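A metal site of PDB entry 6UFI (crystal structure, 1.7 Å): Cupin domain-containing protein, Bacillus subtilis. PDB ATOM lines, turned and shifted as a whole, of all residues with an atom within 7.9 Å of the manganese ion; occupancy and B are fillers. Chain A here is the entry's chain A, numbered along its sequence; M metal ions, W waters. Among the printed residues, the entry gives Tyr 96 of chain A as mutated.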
ATOM      1  N   MET A  84      -9.444 -19.309  -7.455  1.00  0.00           N
ATOM      2  CA  MET A  84      -9.773 -17.912  -7.698  1.00  0.00           C
ATOM      3  C   MET A  84      -8.691 -17.242  -8.546  1.00  0.00           C
ATOM      4  O   MET A  84      -7.504 -17.495  -8.348  1.00  0.00           O
ATOM      5  CB  MET A  84      -9.960 -17.150  -6.380  1.00  0.00           C
ATOM      6  CG  MET A  84     -10.334 -15.676  -6.575  1.00  0.00           C
ATOM      7  SD  MET A  84     -10.836 -14.902  -5.026  1.00  0.00           S
ATOM      8  CE  MET A  84     -12.437 -15.692  -4.769  1.00  0.00           C
ATOM      9  N   ARG A  92     -10.477  -8.696  -4.464  1.00  0.00           N
ATOM     10  CA  ARG A  92     -11.473  -9.530  -3.807  1.00  0.00           C
ATOM     11  C   ARG A  92     -11.950  -8.777  -2.570  1.00  0.00           C
ATOM     12  O   ARG A  92     -11.178  -8.581  -1.619  1.00  0.00           O
ATOM     13  CB  ARG A  92     -10.899 -10.908  -3.452  1.00  0.00           C
ATOM     14  CG  ARG A  92     -11.857 -11.786  -2.615  1.00  0.00           C
ATOM     15  CD  ARG A  92     -13.056 -12.250  -3.414  1.00  0.00           C
ATOM     16  NE  ARG A  92     -13.905 -13.086  -2.541  1.00  0.00           N
ATOM     17  CZ  ARG A  92     -14.906 -12.622  -1.810  1.00  0.00           C
ATOM     18  NH1 ARG A  92     -15.238 -11.340  -1.858  1.00  0.00           N
ATOM     19  NH2 ARG A  92     -15.600 -13.445  -1.029  1.00  0.00           N
ATOM     20  N   GLU A  93     -13.197  -8.338  -2.618  1.00  0.00           N
ATOM     21  CA  GLU A  93     -13.774  -7.399  -1.660  1.00  0.00           C
ATOM     22  C   GLU A  93     -13.585  -7.837  -0.214  1.00  0.00           C
ATOM     23  O   GLU A  93     -13.773  -9.012   0.125  1.00  0.00           O
ATOM     24  CB  GLU A  93     -15.264  -7.242  -1.963  1.00  0.00           C
ATOM     25  CG  GLU A  93     -15.996  -6.426  -0.923  1.00  0.00           C
ATOM     26  CD  GLU A  93     -17.494  -6.316  -1.136  1.00  0.00           C
ATOM     27  OE1 GLU A  93     -18.042  -6.847  -2.124  1.00  0.00           O
ATOM     28  OE2 GLU A  93     -18.135  -5.672  -0.290  1.00  0.00           O
ATOM     29  N   LEU A  94     -13.259  -6.868   0.645  1.00  0.00           N
ATOM     30  CA  LEU A  94     -13.206  -7.051   2.090  1.00  0.00           C
ATOM     31  C   LEU A  94     -14.379  -7.891   2.592  1.00  0.00           C
ATOM     32  O   LEU A  94     -15.543  -7.561   2.340  1.00  0.00           O
ATOM     33  CB  LEU A  94     -13.211  -5.675   2.756  1.00  0.00           C
ATOM     34  CG  LEU A  94     -11.863  -4.944   2.691  1.00  0.00           C
ATOM     35  CD1 LEU A  94     -12.093  -3.435   2.907  1.00  0.00           C
ATOM     36  CD2 LEU A  94     -10.961  -5.514   3.753  1.00  0.00           C
ATOM     37  N   HIS A  95     -14.064  -8.978   3.314  1.00  0.00           N
ATOM     38  CA  HIS A  95     -15.079  -9.946   3.731  1.00  0.00           C
ATOM     39  C   HIS A  95     -14.535 -10.819   4.869  1.00  0.00           C
ATOM     40  O   HIS A  95     -13.362 -10.749   5.235  1.00  0.00           O
ATOM     41  CB  HIS A  95     -15.483 -10.826   2.537  1.00  0.00           C
ATOM     42  CG  HIS A  95     -14.421 -11.782   2.109  1.00  0.00           C
ATOM     43  ND1 HIS A  95     -13.426 -11.437   1.210  1.00  0.00           N
ATOM     44  CD2 HIS A  95     -14.166 -13.062   2.467  1.00  0.00           C
ATOM     45  CE1 HIS A  95     -12.621 -12.467   1.036  1.00  0.00           C
ATOM     46  NE2 HIS A  95     -13.041 -13.458   1.793  1.00  0.00           N
ATOM     47  N   TYR A  96     -15.412 -11.657   5.425  1.00  0.00           N
ATOM     48  CA  TYR A  96     -14.967 -12.686   6.372  1.00  0.00           C
ATOM     49  C   TYR A  96     -15.884 -13.889   6.237  1.00  0.00           C
ATOM     50  O   TYR A  96     -16.916 -13.837   5.576  1.00  0.00           O
ATOM     51  CB  TYR A  96     -14.954 -12.158   7.821  1.00  0.00           C
ATOM     52  CG  TYR A  96     -16.308 -11.737   8.368  1.00  0.00           C
ATOM     53  CD1 TYR A  96     -17.135 -12.654   8.999  1.00  0.00           C
ATOM     54  CD2 TYR A  96     -16.735 -10.416   8.267  1.00  0.00           C
ATOM     55  CE1 TYR A  96     -18.383 -12.257   9.525  1.00  0.00           C
ATOM     56  CE2 TYR A  96     -17.970 -10.006   8.782  1.00  0.00           C
ATOM     57  CZ  TYR A  96     -18.790 -10.949   9.397  1.00  0.00           C
ATOM     58  OH  TYR A  96     -20.018 -10.584   9.910  1.00  0.00           O
ATOM     59  N   HIS A  97     -15.492 -14.991   6.875  1.00  0.00           N
ATOM     60  CA  HIS A  97     -16.203 -16.265   6.770  1.00  0.00           C
ATOM     61  C   HIS A  97     -16.285 -16.891   8.159  1.00  0.00           C
ATOM     62  O   HIS A  97     -15.492 -16.585   9.040  1.00  0.00           O
ATOM     63  CB  HIS A  97     -15.514 -17.342   5.880  1.00  0.00           C
ATOM     64  CG  HIS A  97     -14.717 -16.830   4.721  1.00  0.00           C
ATOM     65  ND1 HIS A  97     -15.277 -16.611   3.488  1.00  0.00           N
ATOM     66  CD2 HIS A  97     -13.386 -16.620   4.574  1.00  0.00           C
ATOM     67  CE1 HIS A  97     -14.335 -16.211   2.645  1.00  0.00           C
ATOM     68  NE2 HIS A  97     -13.182 -16.202   3.284  1.00  0.00           N
ATOM     69  N   GLU A  99     -15.582 -20.043   8.318  1.00  0.00           N
ATOM     70  CA  GLU A  99     -14.489 -20.991   8.175  1.00  0.00           C
ATOM     71  C   GLU A  99     -13.128 -20.302   8.223  1.00  0.00           C
ATOM     72  O   GLU A  99     -12.971 -19.140   7.841  1.00  0.00           O
ATOM     73  CB  GLU A  99     -14.608 -21.732   6.850  1.00  0.00           C
ATOM     74  CG  GLU A  99     -15.891 -22.564   6.697  1.00  0.00           C
ATOM     75  CD  GLU A  99     -17.115 -21.755   6.281  1.00  0.00           C
ATOM     76  OE1 GLU A  99     -17.041 -20.509   6.161  1.00  0.00           O
ATOM     77  OE2 GLU A  99     -18.175 -22.365   6.007  1.00  0.00           O
ATOM     78  N   ALA A 100     -12.120 -21.055   8.683  1.00  0.00           N
ATOM     79  CA  ALA A 100     -10.729 -20.670   8.458  1.00  0.00           C
ATOM     80  C   ALA A 100     -10.400 -20.864   6.984  1.00  0.00           C
ATOM     81  O   ALA A 100     -10.966 -21.743   6.319  1.00  0.00           O
ATOM     82  CB  ALA A 100      -9.776 -21.508   9.314  1.00  0.00           C
ATOM     83  N   GLU A 101      -9.482 -20.046   6.477  1.00  0.00           N
ATOM     84  CA  GLU A 101      -9.095 -20.058   5.076  1.00  0.00           C
ATOM     85  C   GLU A 101      -7.597 -20.242   4.972  1.00  0.00           C
ATOM     86  O   GLU A 101      -6.834 -19.498   5.598  1.00  0.00           O
ATOM     87  CB  GLU A 101      -9.509 -18.747   4.395  1.00  0.00           C
ATOM     88  CG  GLU A 101      -8.903 -18.536   3.009  1.00  0.00           C
ATOM     89  CD  GLU A 101      -9.409 -17.261   2.388  1.00  0.00           C
ATOM     90  OE1 GLU A 101     -10.599 -16.945   2.585  1.00  0.00           O
ATOM     91  OE2 GLU A 101      -8.615 -16.558   1.707  1.00  0.00           O
ATOM     92  N   TRP A 102      -7.175 -21.225   4.172  1.00  0.00           N
ATOM     93  CA  TRP A 102      -5.783 -21.464   3.840  1.00  0.00           C
ATOM     94  C   TRP A 102      -5.604 -21.257   2.333  1.00  0.00           C
ATOM     95  O   TRP A 102      -6.521 -21.550   1.557  1.00  0.00           O
ATOM     96  CB  TRP A 102      -5.406 -22.902   4.243  1.00  0.00           C
ATOM     97  CG  TRP A 102      -3.985 -23.346   3.984  1.00  0.00           C
ATOM     98  CD1 TRP A 102      -2.949 -23.376   4.882  1.00  0.00           C
ATOM     99  CD2 TRP A 102      -3.471 -23.879   2.765  1.00  0.00           C
ATOM    100  NE1 TRP A 102      -1.821 -23.896   4.289  1.00  0.00           N
ATOM    101  CE2 TRP A 102      -2.111 -24.211   2.990  1.00  0.00           C
ATOM    102  CE3 TRP A 102      -4.017 -24.106   1.495  1.00  0.00           C
ATOM    103  CZ2 TRP A 102      -1.292 -24.746   1.986  1.00  0.00           C
ATOM    104  CZ3 TRP A 102      -3.196 -24.654   0.495  1.00  0.00           C
ATOM    105  CH2 TRP A 102      -1.852 -24.961   0.756  1.00  0.00           C
ATOM    106  N   TRP A 132      -1.101 -18.224   2.737  1.00  0.00           N
ATOM    107  CA  TRP A 132      -1.660 -17.455   3.848  1.00  0.00           C
ATOM    108  C   TRP A 132      -2.642 -18.331   4.618  1.00  0.00           C
ATOM    109  O   TRP A 132      -3.052 -19.386   4.144  1.00  0.00           O
ATOM    110  CB  TRP A 132      -2.322 -16.138   3.390  1.00  0.00           C
ATOM    111  CG  TRP A 132      -3.572 -16.193   2.544  1.00  0.00           C
ATOM    112  CD1 TRP A 132      -4.838 -16.573   2.933  1.00  0.00           C
ATOM    113  CD2 TRP A 132      -3.694 -15.760   1.177  1.00  0.00           C
ATOM    114  NE1 TRP A 132      -5.722 -16.425   1.875  1.00  0.00           N
ATOM    115  CE2 TRP A 132      -5.040 -15.922   0.798  1.00  0.00           C
ATOM    116  CE3 TRP A 132      -2.771 -15.268   0.241  1.00  0.00           C
ATOM    117  CZ2 TRP A 132      -5.496 -15.612  -0.492  1.00  0.00           C
ATOM    118  CZ3 TRP A 132      -3.229 -14.956  -1.024  1.00  0.00           C
ATOM    119  CH2 TRP A 132      -4.573 -15.126  -1.383  1.00  0.00           C
ATOM    120  N   PHE A 134      -6.025 -17.432   7.250  1.00  0.00           N
ATOM    121  CA  PHE A 134      -6.863 -16.462   7.939  1.00  0.00           C
ATOM    122  C   PHE A 134      -7.763 -17.207   8.905  1.00  0.00           C
ATOM    123  O   PHE A 134      -8.642 -17.960   8.471  1.00  0.00           O
ATOM    124  CB  PHE A 134      -7.713 -15.660   6.945  1.00  0.00           C
ATOM    125  CG  PHE A 134      -6.923 -14.902   5.906  1.00  0.00           C
ATOM    126  CD1 PHE A 134      -5.661 -14.399   6.197  1.00  0.00           C
ATOM    127  CD2 PHE A 134      -7.447 -14.696   4.639  1.00  0.00           C
ATOM    128  CE1 PHE A 134      -4.937 -13.685   5.220  1.00  0.00           C
ATOM    129  CE2 PHE A 134      -6.747 -13.986   3.664  1.00  0.00           C
ATOM    130  CZ  PHE A 134      -5.482 -13.471   3.963  1.00  0.00           C
ATOM    131  N   LEU A 138     -11.973 -13.724  10.937  1.00  0.00           N
ATOM    132  CA  LEU A 138     -11.191 -12.479  10.872  1.00  0.00           C
ATOM    133  C   LEU A 138     -11.274 -11.901   9.464  1.00  0.00           C
ATOM    134  O   LEU A 138     -11.183 -12.629   8.469  1.00  0.00           O
ATOM    135  CB  LEU A 138      -9.729 -12.742  11.259  1.00  0.00           C
ATOM    136  CG  LEU A 138      -9.533 -13.244  12.714  1.00  0.00           C
ATOM    137  CD1 LEU A 138      -8.047 -13.362  13.041  1.00  0.00           C
ATOM    138  CD2 LEU A 138     -10.237 -12.315  13.713  1.00  0.00           C
ATOM    139  N   PRO A 139     -11.487 -10.592   9.358  1.00  0.00           N
ATOM    140  CA  PRO A 139     -11.804  -9.994   8.051  1.00  0.00           C
ATOM    141  C   PRO A 139     -10.553  -9.719   7.221  1.00  0.00           C
ATOM    142  O   PRO A 139      -9.505  -9.343   7.746  1.00  0.00           O
ATOM    143  CB  PRO A 139     -12.521  -8.706   8.429  1.00  0.00           C
ATOM    144  CG  PRO A 139     -11.836  -8.289   9.729  1.00  0.00           C
ATOM    145  CD  PRO A 139     -11.603  -9.611  10.459  1.00  0.00           C
ATOM    146  N   HIS A 140     -10.678  -9.908   5.907  1.00  0.00           N
ATOM    147  CA  HIS A 140      -9.508  -9.874   5.044  1.00  0.00           C
ATOM    148  C   HIS A 140      -9.888  -9.437   3.638  1.00  0.00           C
ATOM    149  O   HIS A 140     -11.062  -9.311   3.289  1.00  0.00           O
ATOM    150  CB  HIS A 140      -8.814 -11.252   5.031  1.00  0.00           C
ATOM    151  CG  HIS A 140      -9.741 -12.396   4.722  1.00  0.00           C
ATOM    152  ND1 HIS A 140     -10.452 -13.073   5.691  1.00  0.00           N
ATOM    153  CD2 HIS A 140     -10.043 -13.001   3.541  1.00  0.00           C
ATOM    154  CE1 HIS A 140     -11.161 -14.037   5.124  1.00  0.00           C
ATOM    155  NE2 HIS A 140     -10.928 -14.014   3.822  1.00  0.00           N
ATOM    156  N   SER A 141      -8.865  -9.211   2.818  1.00  0.00           N
ATOM    157  CA  SER A 141      -9.014  -8.842   1.414  1.00  0.00           C
ATOM    158  C   SER A 141      -7.831  -9.375   0.645  1.00  0.00           C
ATOM    159  O   SER A 141      -6.797  -9.721   1.228  1.00  0.00           O
ATOM    160  CB  SER A 141      -9.118  -7.321   1.246  1.00  0.00           C
ATOM    161  OG  SER A 141      -7.883  -6.723   1.627  1.00  0.00           O
ATOM    162  N   ILE A 142      -7.966  -9.426  -0.682  1.00  0.00           N
ATOM    163  CA  ILE A 142      -6.890  -9.806  -1.606  1.00  0.00           C
ATOM    164  C   ILE A 142      -6.885  -8.799  -2.737  1.00  0.00           C
ATOM    165  O   ILE A 142      -7.949  -8.467  -3.276  1.00  0.00           O
ATOM    166  CB  ILE A 142      -7.078 -11.219  -2.182  1.00  0.00           C
ATOM    167  CG1 ILE A 142      -7.488 -12.238  -1.121  1.00  0.00           C
ATOM    168  CG2 ILE A 142      -5.819 -11.674  -2.903  1.00  0.00           C
ATOM    169  CD1 ILE A 142      -8.139 -13.479  -1.727  1.00  0.00           C
ATOM    170  N   LEU A 153      -7.763 -21.658  -2.673  1.00  0.00           N
ATOM    171  CA  LEU A 153      -8.211 -21.441  -1.306  1.00  0.00           C
ATOM    172  C   LEU A 153      -8.782 -22.746  -0.774  1.00  0.00           C
ATOM    173  O   LEU A 153      -9.452 -23.485  -1.504  1.00  0.00           O
ATOM    174  CB  LEU A 153      -9.284 -20.366  -1.247  1.00  0.00           C
ATOM    175  CG  LEU A 153      -8.955 -19.032  -1.908  1.00  0.00           C
ATOM    176  CD1 LEU A 153     -10.160 -18.119  -1.846  1.00  0.00           C
ATOM    177  CD2 LEU A 153      -7.751 -18.386  -1.223  1.00  0.00           C
ATOM    178  N   PHE A 155     -10.996 -24.178   2.640  1.00  0.00           N
ATOM    179  CA  PHE A 155     -11.779 -23.765   3.797  1.00  0.00           C
ATOM    180  C   PHE A 155     -12.074 -24.977   4.658  1.00  0.00           C
ATOM    181  O   PHE A 155     -12.334 -26.066   4.134  1.00  0.00           O
ATOM    182  CB  PHE A 155     -13.096 -23.119   3.358  1.00  0.00           C
ATOM    183  CG  PHE A 155     -12.877 -21.930   2.497  1.00  0.00           C
ATOM    184  CD1 PHE A 155     -12.707 -20.681   3.071  1.00  0.00           C
ATOM    185  CD2 PHE A 155     -12.799 -22.049   1.117  1.00  0.00           C
ATOM    186  CE1 PHE A 155     -12.476 -19.551   2.273  1.00  0.00           C
ATOM    187  CE2 PHE A 155     -12.549 -20.932   0.317  1.00  0.00           C
ATOM    188  CZ  PHE A 155     -12.398 -19.689   0.907  1.00  0.00           C
ATOM    189  N   PHE A 160     -18.972 -25.230   2.726  1.00  0.00           N
ATOM    190  CA  PHE A 160     -18.717 -23.864   2.284  1.00  0.00           C
ATOM    191  C   PHE A 160     -19.661 -23.475   1.141  1.00  0.00           C
ATOM    192  O   PHE A 160     -19.766 -24.185   0.136  1.00  0.00           O
ATOM    193  CB  PHE A 160     -17.250 -23.744   1.826  1.00  0.00           C
ATOM    194  CG  PHE A 160     -16.855 -22.359   1.402  1.00  0.00           C
ATOM    195  CD1 PHE A 160     -16.454 -21.416   2.340  1.00  0.00           C
ATOM    196  CD2 PHE A 160     -16.844 -22.014   0.055  1.00  0.00           C
ATOM    197  CE1 PHE A 160     -16.068 -20.138   1.943  1.00  0.00           C
ATOM    198  CE2 PHE A 160     -16.467 -20.740  -0.347  1.00  0.00           C
ATOM    199  CZ  PHE A 160     -16.077 -19.806   0.595  1.00  0.00           C
ATOM    200  N   THR A 165     -20.065 -16.503   3.746  1.00  0.00           N
ATOM    201  CA  THR A 165     -19.216 -15.330   3.483  1.00  0.00           C
ATOM    202  C   THR A 165     -19.979 -14.015   3.620  1.00  0.00           C
ATOM    203  O   THR A 165     -21.018 -13.825   2.983  1.00  0.00           O
ATOM    204  CB  THR A 165     -18.589 -15.402   2.105  1.00  0.00           C
ATOM    205  OG1 THR A 165     -17.801 -16.598   1.991  1.00  0.00           O
ATOM    206  CG2 THR A 165     -17.692 -14.203   1.910  1.00  0.00           C
ATOM    207  N   GLN A 167     -19.750 -10.012   3.102  1.00  0.00           N
ATOM    208  CA  GLN A 167     -19.087  -8.941   2.373  1.00  0.00           C
ATOM    209  C   GLN A 167     -19.389  -7.570   2.992  1.00  0.00           C
ATOM    210  O   GLN A 167     -20.532  -7.296   3.349  1.00  0.00           O
ATOM    211  CB  GLN A 167     -19.539  -8.918   0.911  1.00  0.00           C
ATOM    212  CG  GLN A 167     -18.521  -9.455  -0.058  1.00  0.00           C
ATOM    213  CD  GLN A 167     -18.452 -10.964  -0.052  1.00  0.00           C
ATOM    214  OE1 GLN A 167     -17.365 -11.543  -0.009  1.00  0.00           O
ATOM    215  NE2 GLN A 167     -19.614 -11.600  -0.104  1.00  0.00           N
HETATM  216 MN    MN M   1     -11.836 -15.276   2.216  1.00  0.00          MN
HETATM  217  O   HOH W   1     -12.736 -16.009  -0.017  1.00  0.00           O
HETATM  218  O   HOH W   2     -10.325 -14.682   0.738  1.00  0.00           O
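Four residues have an atom within 4 Å of the manganese ion: His 95, His 97, Glu 101 and His 140.
The manganese ion is bound by a ring nitrogen (NE2) of His 97 (2.0 Å), the side-chain carboxylate of Glu 101 (2.1 Å), water W2 (2.2 Å), a ring nitrogen (NE2) of His 95 (2.2 Å), a ring nitrogen (NE2) of His 140 (2.2 Å) and water W1 (2.5 Å).
The manganese ion has six donor atoms within binding distance.
ND1 of His 97 is in hydrogen-bond range of OG1 of Thr 165 (2.9 Å).
The backbone carbonyl oxygen of Glu 93 is in hydrogen-bond range of a ring nitrogen (ND1) of His 95, 2.7 Å away.
The indole nitrogen (NE1) of Trp 132 is in hydrogen-bond range of the side-chain carboxylate (OE2) of Glu 101.
N of Phe 134 lies within hydrogen-bond range of O of Glu 101 (2.8 Å).
The backbone carbonyl oxygen (O) of Leu 138 lies within hydrogen-bond range of a ring nitrogen (ND1) of His 140, at 2.9 Å.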
